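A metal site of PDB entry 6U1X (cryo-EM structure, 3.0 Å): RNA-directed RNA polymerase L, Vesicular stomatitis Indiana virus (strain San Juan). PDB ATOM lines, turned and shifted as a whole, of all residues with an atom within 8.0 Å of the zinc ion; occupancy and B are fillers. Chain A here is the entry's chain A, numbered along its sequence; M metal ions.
The zinc ion is bound by ND1 of His 1294 (2.0 Å), NE2 of His 1296 (2.0 Å), SG of Cys 1123 (2.2 Å) and SG of Cys 1120 (2.3 Å).
Of the 21 residues printed, 4 come within 4 Å of the zinc ion. Along chain A the residues within 4 Å of the zinc ion span positions 1120 to 1296.
The backbone NH of His 1114 lies within hydrogen-bond range of the backbone carbonyl oxygen of His 1294. The side-chain carboxylate (OE2) of Glu 1731 is in hydrogen-bond range of a ring nitrogen (NE2) of His 1294.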
ATOM      1  N   HIS A1114       2.903 -32.363  -4.727  1.00  0.00           N
ATOM      2  CA  HIS A1114       2.497 -32.773  -6.070  1.00  0.00           C
ATOM      3  C   HIS A1114       3.697 -33.449  -6.721  1.00  0.00           C
ATOM      4  O   HIS A1114       4.630 -32.777  -7.168  1.00  0.00           O
ATOM      5  CB  HIS A1114       2.006 -31.595  -6.899  1.00  0.00           C
ATOM      6  CG  HIS A1114       0.808 -30.906  -6.325  1.00  0.00           C
ATOM      7  ND1 HIS A1114      -0.441 -31.490  -6.313  1.00  0.00           N
ATOM      8  CD2 HIS A1114       0.663 -29.698  -5.746  1.00  0.00           C
ATOM      9  CE1 HIS A1114      -1.297 -30.655  -5.749  1.00  0.00           C
ATOM     10  NE2 HIS A1114      -0.653 -29.567  -5.399  1.00  0.00           N
ATOM     11  N   ARG A1115       3.667 -34.778  -6.776  1.00  0.00           N
ATOM     12  CA  ARG A1115       4.796 -35.522  -7.322  1.00  0.00           C
ATOM     13  C   ARG A1115       4.920 -35.316  -8.821  1.00  0.00           C
ATOM     14  O   ARG A1115       3.939 -35.073  -9.527  1.00  0.00           O
ATOM     15  CB  ARG A1115       4.662 -37.008  -6.991  1.00  0.00           C
ATOM     16  CG  ARG A1115       3.321 -37.649  -7.332  1.00  0.00           C
ATOM     17  CD  ARG A1115       3.315 -39.124  -6.990  1.00  0.00           C
ATOM     18  NE  ARG A1115       3.550 -39.358  -5.562  1.00  0.00           N
ATOM     19  CZ  ARG A1115       3.667 -40.553  -5.006  1.00  0.00           C
ATOM     20  NH1 ARG A1115       3.571 -41.666  -5.733  1.00  0.00           N
ATOM     21  NH2 ARG A1115       3.877 -40.650  -3.704  1.00  0.00           N
ATOM     22  N   LYS A1116       6.153 -35.411  -9.308  1.00  0.00           N
ATOM     23  CA  LYS A1116       6.467 -35.060 -10.686  1.00  0.00           C
ATOM     24  C   LYS A1116       6.118 -36.180 -11.662  1.00  0.00           C
ATOM     25  O   LYS A1116       5.821 -35.898 -12.832  1.00  0.00           O
ATOM     26  CB  LYS A1116       7.946 -34.695 -10.802  1.00  0.00           C
ATOM     27  CG  LYS A1116       8.407 -34.167 -12.148  1.00  0.00           C
ATOM     28  CD  LYS A1116       7.835 -32.789 -12.438  1.00  0.00           C
ATOM     29  CE  LYS A1116       8.415 -32.226 -13.717  1.00  0.00           C
ATOM     30  NZ  LYS A1116       7.783 -30.942 -14.095  1.00  0.00           N
ATOM     31  N   THR A1118       3.458 -37.965 -11.568  1.00  0.00           N
ATOM     32  CA  THR A1118       2.129 -37.508 -11.918  1.00  0.00           C
ATOM     33  C   THR A1118       2.259 -36.284 -12.825  1.00  0.00           C
ATOM     34  O   THR A1118       3.223 -35.527 -12.696  1.00  0.00           O
ATOM     35  CB  THR A1118       1.349 -37.173 -10.646  1.00  0.00           C
ATOM     36  OG1 THR A1118       1.341 -38.310  -9.783  1.00  0.00           O
ATOM     37  CG2 THR A1118      -0.087 -36.800 -10.952  1.00  0.00           C
ATOM     38  N   PRO A1119       1.315 -36.062 -13.749  1.00  0.00           N
ATOM     39  CA  PRO A1119       1.448 -34.913 -14.659  1.00  0.00           C
ATOM     40  C   PRO A1119       1.628 -33.556 -13.977  1.00  0.00           C
ATOM     41  O   PRO A1119       2.038 -32.611 -14.653  1.00  0.00           O
ATOM     42  CB  PRO A1119       0.150 -34.965 -15.465  1.00  0.00           C
ATOM     43  CG  PRO A1119      -0.150 -36.403 -15.539  1.00  0.00           C
ATOM     44  CD  PRO A1119       0.231 -36.964 -14.204  1.00  0.00           C
ATOM     45  N   CYS A1120       1.355 -33.448 -12.678  1.00  0.00           N
ATOM     46  CA  CYS A1120       1.614 -32.215 -11.921  1.00  0.00           C
ATOM     47  C   CYS A1120       0.873 -31.029 -12.547  1.00  0.00           C
ATOM     48  O   CYS A1120       1.457 -30.054 -13.024  1.00  0.00           O
ATOM     49  CB  CYS A1120       3.115 -31.943 -11.833  1.00  0.00           C
ATOM     50  SG  CYS A1120       3.574 -30.721 -10.575  1.00  0.00           S
ATOM     51  N   ALA A1121      -0.459 -31.162 -12.534  1.00  0.00           N
ATOM     52  CA  ALA A1121      -1.382 -30.193 -13.136  1.00  0.00           C
ATOM     53  C   ALA A1121      -1.016 -28.728 -12.935  1.00  0.00           C
ATOM     54  O   ALA A1121      -1.025 -27.980 -13.921  1.00  0.00           O
ATOM     55  CB  ALA A1121      -2.787 -30.458 -12.588  1.00  0.00           C
ATOM     56  N   PRO A1122      -0.697 -28.243 -11.721  1.00  0.00           N
ATOM     57  CA  PRO A1122      -0.429 -26.806 -11.566  1.00  0.00           C
ATOM     58  C   PRO A1122       0.835 -26.304 -12.234  1.00  0.00           C
ATOM     59  O   PRO A1122       1.139 -25.116 -12.120  1.00  0.00           O
ATOM     60  CB  PRO A1122      -0.352 -26.632 -10.046  1.00  0.00           C
ATOM     61  CG  PRO A1122      -0.064 -27.969  -9.515  1.00  0.00           C
ATOM     62  CD  PRO A1122      -0.750 -28.924 -10.418  1.00  0.00           C
ATOM     63  N   CYS A1123       1.595 -27.159 -12.930  1.00  0.00           N
ATOM     64  CA  CYS A1123       2.733 -26.700 -13.718  1.00  0.00           C
ATOM     65  C   CYS A1123       2.328 -26.185 -15.097  1.00  0.00           C
ATOM     66  O   CYS A1123       3.204 -25.745 -15.852  1.00  0.00           O
ATOM     67  CB  CYS A1123       3.761 -27.811 -13.872  1.00  0.00           C
ATOM     68  SG  CYS A1123       4.922 -27.932 -12.500  1.00  0.00           S
ATOM     69  N   ASN A1124       1.041 -26.233 -15.431  1.00  0.00           N
ATOM     70  CA  ASN A1124       0.529 -25.692 -16.691  1.00  0.00           C
ATOM     71  C   ASN A1124      -0.168 -24.347 -16.506  1.00  0.00           C
ATOM     72  O   ASN A1124      -0.014 -23.460 -17.345  1.00  0.00           O
ATOM     73  CB  ASN A1124      -0.434 -26.683 -17.333  1.00  0.00           C
ATOM     74  CG  ASN A1124       0.186 -28.048 -17.544  1.00  0.00           C
ATOM     75  OD1 ASN A1124      -0.381 -29.066 -17.146  1.00  0.00           O
ATOM     76  ND2 ASN A1124       1.352 -28.069 -18.182  1.00  0.00           N
ATOM     77  N   SER A1126       0.531 -22.108 -14.345  1.00  0.00           N
ATOM     78  CA  SER A1126       1.444 -21.101 -13.831  1.00  0.00           C
ATOM     79  C   SER A1126       2.876 -21.522 -14.143  1.00  0.00           C
ATOM     80  O   SER A1126       3.113 -22.546 -14.790  1.00  0.00           O
ATOM     81  CB  SER A1126       1.236 -20.897 -12.329  1.00  0.00           C
ATOM     82  OG  SER A1126       1.933 -19.748 -11.861  1.00  0.00           O
ATOM     83  N   GLY A1127       3.826 -20.723 -13.670  1.00  0.00           N
ATOM     84  CA  GLY A1127       5.232 -20.949 -13.923  1.00  0.00           C
ATOM     85  C   GLY A1127       6.047 -21.134 -12.657  1.00  0.00           C
ATOM     86  O   GLY A1127       5.688 -21.936 -11.796  1.00  0.00           O
ATOM     87  N   ASN A1129       6.659 -20.641  -9.446  1.00  0.00           N
ATOM     88  CA  ASN A1129       6.082 -20.188  -8.187  1.00  0.00           C
ATOM     89  C   ASN A1129       6.157 -21.250  -7.109  1.00  0.00           C
ATOM     90  O   ASN A1129       5.368 -21.222  -6.158  1.00  0.00           O
ATOM     91  CB  ASN A1129       4.624 -19.776  -8.378  1.00  0.00           C
ATOM     92  CG  ASN A1129       3.736 -20.958  -8.733  1.00  0.00           C
ATOM     93  OD1 ASN A1129       4.200 -21.944  -9.297  1.00  0.00           O
ATOM     94  ND2 ASN A1129       2.462 -20.862  -8.386  1.00  0.00           N
ATOM     95  N   TYR A1130       7.078 -22.211  -7.228  1.00  0.00           N
ATOM     96  CA  TYR A1130       7.037 -23.438  -6.453  1.00  0.00           C
ATOM     97  C   TYR A1130       8.404 -23.750  -5.850  1.00  0.00           C
ATOM     98  O   TYR A1130       9.411 -23.109  -6.160  1.00  0.00           O
ATOM     99  CB  TYR A1130       6.578 -24.609  -7.325  1.00  0.00           C
ATOM    100  CG  TYR A1130       7.438 -24.842  -8.547  1.00  0.00           C
ATOM    101  CD1 TYR A1130       7.195 -24.158  -9.727  1.00  0.00           C
ATOM    102  CD2 TYR A1130       8.485 -25.750  -8.529  1.00  0.00           C
ATOM    103  CE1 TYR A1130       7.968 -24.361 -10.844  1.00  0.00           C
ATOM    104  CE2 TYR A1130       9.262 -25.970  -9.647  1.00  0.00           C
ATOM    105  CZ  TYR A1130       9.003 -25.273 -10.801  1.00  0.00           C
ATOM    106  OH  TYR A1130       9.770 -25.483 -11.914  1.00  0.00           O
ATOM    107  N   VAL A1131       8.398 -24.758  -4.980  1.00  0.00           N
ATOM    108  CA  VAL A1131       9.606 -25.300  -4.368  1.00  0.00           C
ATOM    109  C   VAL A1131       9.728 -26.740  -4.814  1.00  0.00           C
ATOM    110  O   VAL A1131       8.797 -27.540  -4.628  1.00  0.00           O
ATOM    111  CB  VAL A1131       9.559 -25.198  -2.835  1.00  0.00           C
ATOM    112  CG1 VAL A1131      10.899 -25.572  -2.232  1.00  0.00           C
ATOM    113  CG2 VAL A1131       9.151 -23.810  -2.407  1.00  0.00           C
ATOM    114  N   SER A1132      10.867 -27.086  -5.392  1.00  0.00           N
ATOM    115  CA  SER A1132      11.155 -28.444  -5.844  1.00  0.00           C
ATOM    116  C   SER A1132      12.053 -29.144  -4.831  1.00  0.00           C
ATOM    117  O   SER A1132      12.900 -28.522  -4.191  1.00  0.00           O
ATOM    118  CB  SER A1132      11.822 -28.440  -7.212  1.00  0.00           C
ATOM    119  OG  SER A1132      11.810 -29.736  -7.783  1.00  0.00           O
ATOM    120  N   ASP A1293       9.524 -33.910  -6.120  1.00  0.00           N
ATOM    121  CA  ASP A1293       8.250 -33.405  -5.640  1.00  0.00           C
ATOM    122  C   ASP A1293       8.201 -31.892  -5.787  1.00  0.00           C
ATOM    123  O   ASP A1293       9.233 -31.219  -5.710  1.00  0.00           O
ATOM    124  CB  ASP A1293       8.007 -33.783  -4.175  1.00  0.00           C
ATOM    125  CG  ASP A1293       7.774 -35.265  -3.990  1.00  0.00           C
ATOM    126  OD1 ASP A1293       7.854 -36.009  -4.989  1.00  0.00           O
ATOM    127  OD2 ASP A1293       7.497 -35.688  -2.846  1.00  0.00           O
ATOM    128  N   HIS A1294       6.997 -31.374  -6.015  1.00  0.00           N
ATOM    129  CA  HIS A1294       6.754 -29.954  -6.164  1.00  0.00           C
ATOM    130  C   HIS A1294       5.808 -29.469  -5.079  1.00  0.00           C
ATOM    131  O   HIS A1294       4.936 -30.205  -4.604  1.00  0.00           O
ATOM    132  CB  HIS A1294       6.136 -29.631  -7.523  1.00  0.00           C
ATOM    133  CG  HIS A1294       7.112 -29.662  -8.661  1.00  0.00           C
ATOM    134  ND1 HIS A1294       6.770 -29.254  -9.929  1.00  0.00           N
ATOM    135  CD2 HIS A1294       8.405 -30.040  -8.716  1.00  0.00           C
ATOM    136  CE1 HIS A1294       7.818 -29.388 -10.726  1.00  0.00           C
ATOM    137  NE2 HIS A1294       8.819 -29.858 -10.015  1.00  0.00           N
ATOM    138  N   TYR A1295       5.983 -28.213  -4.698  1.00  0.00           N
ATOM    139  CA  TYR A1295       5.132 -27.532  -3.733  1.00  0.00           C
ATOM    140  C   TYR A1295       4.760 -26.192  -4.361  1.00  0.00           C
ATOM    141  O   TYR A1295       5.578 -25.261  -4.374  1.00  0.00           O
ATOM    142  CB  TYR A1295       5.822 -27.345  -2.387  1.00  0.00           C
ATOM    143  CG  TYR A1295       6.141 -28.652  -1.699  1.00  0.00           C
ATOM    144  CD1 TYR A1295       5.344 -29.124  -0.668  1.00  0.00           C
ATOM    145  CD2 TYR A1295       7.223 -29.423  -2.081  1.00  0.00           C
ATOM    146  CE1 TYR A1295       5.613 -30.309  -0.041  1.00  0.00           C
ATOM    147  CE2 TYR A1295       7.506 -30.612  -1.463  1.00  0.00           C
ATOM    148  CZ  TYR A1295       6.705 -31.055  -0.437  1.00  0.00           C
ATOM    149  OH  TYR A1295       6.988 -32.243   0.180  1.00  0.00           O
ATOM    150  N   HIS A1296       3.552 -26.108  -4.906  1.00  0.00           N
ATOM    151  CA  HIS A1296       3.046 -24.926  -5.565  1.00  0.00           C
ATOM    152  C   HIS A1296       2.136 -24.147  -4.613  1.00  0.00           C
ATOM    153  O   HIS A1296       1.549 -24.708  -3.683  1.00  0.00           O
ATOM    154  CB  HIS A1296       2.269 -25.280  -6.831  1.00  0.00           C
ATOM    155  CG  HIS A1296       3.055 -26.054  -7.837  1.00  0.00           C
ATOM    156  ND1 HIS A1296       3.703 -25.455  -8.891  1.00  0.00           N
ATOM    157  CD2 HIS A1296       3.272 -27.381  -7.975  1.00  0.00           C
ATOM    158  CE1 HIS A1296       4.300 -26.377  -9.625  1.00  0.00           C
ATOM    159  NE2 HIS A1296       4.049 -27.555  -9.085  1.00  0.00           N
ATOM    160  N   GLU A1731      14.695 -32.899 -13.146  1.00  0.00           N
ATOM    161  CA  GLU A1731      13.505 -33.196 -12.350  1.00  0.00           C
ATOM    162  C   GLU A1731      12.928 -34.571 -12.659  1.00  0.00           C
ATOM    163  O   GLU A1731      11.888 -34.926 -12.077  1.00  0.00           O
ATOM    164  CB  GLU A1731      12.438 -32.119 -12.583  1.00  0.00           C
ATOM    165  CG  GLU A1731      12.601 -30.887 -11.714  1.00  0.00           C
ATOM    166  CD  GLU A1731      11.652 -29.778 -12.098  1.00  0.00           C
ATOM    167  OE1 GLU A1731      10.989 -29.888 -13.152  1.00  0.00           O
ATOM    168  OE2 GLU A1731      11.580 -28.780 -11.348  1.00  0.00           O
HETATM  169 ZN    ZN M   1       4.853 -28.832 -10.448  1.00  0.00          ZN
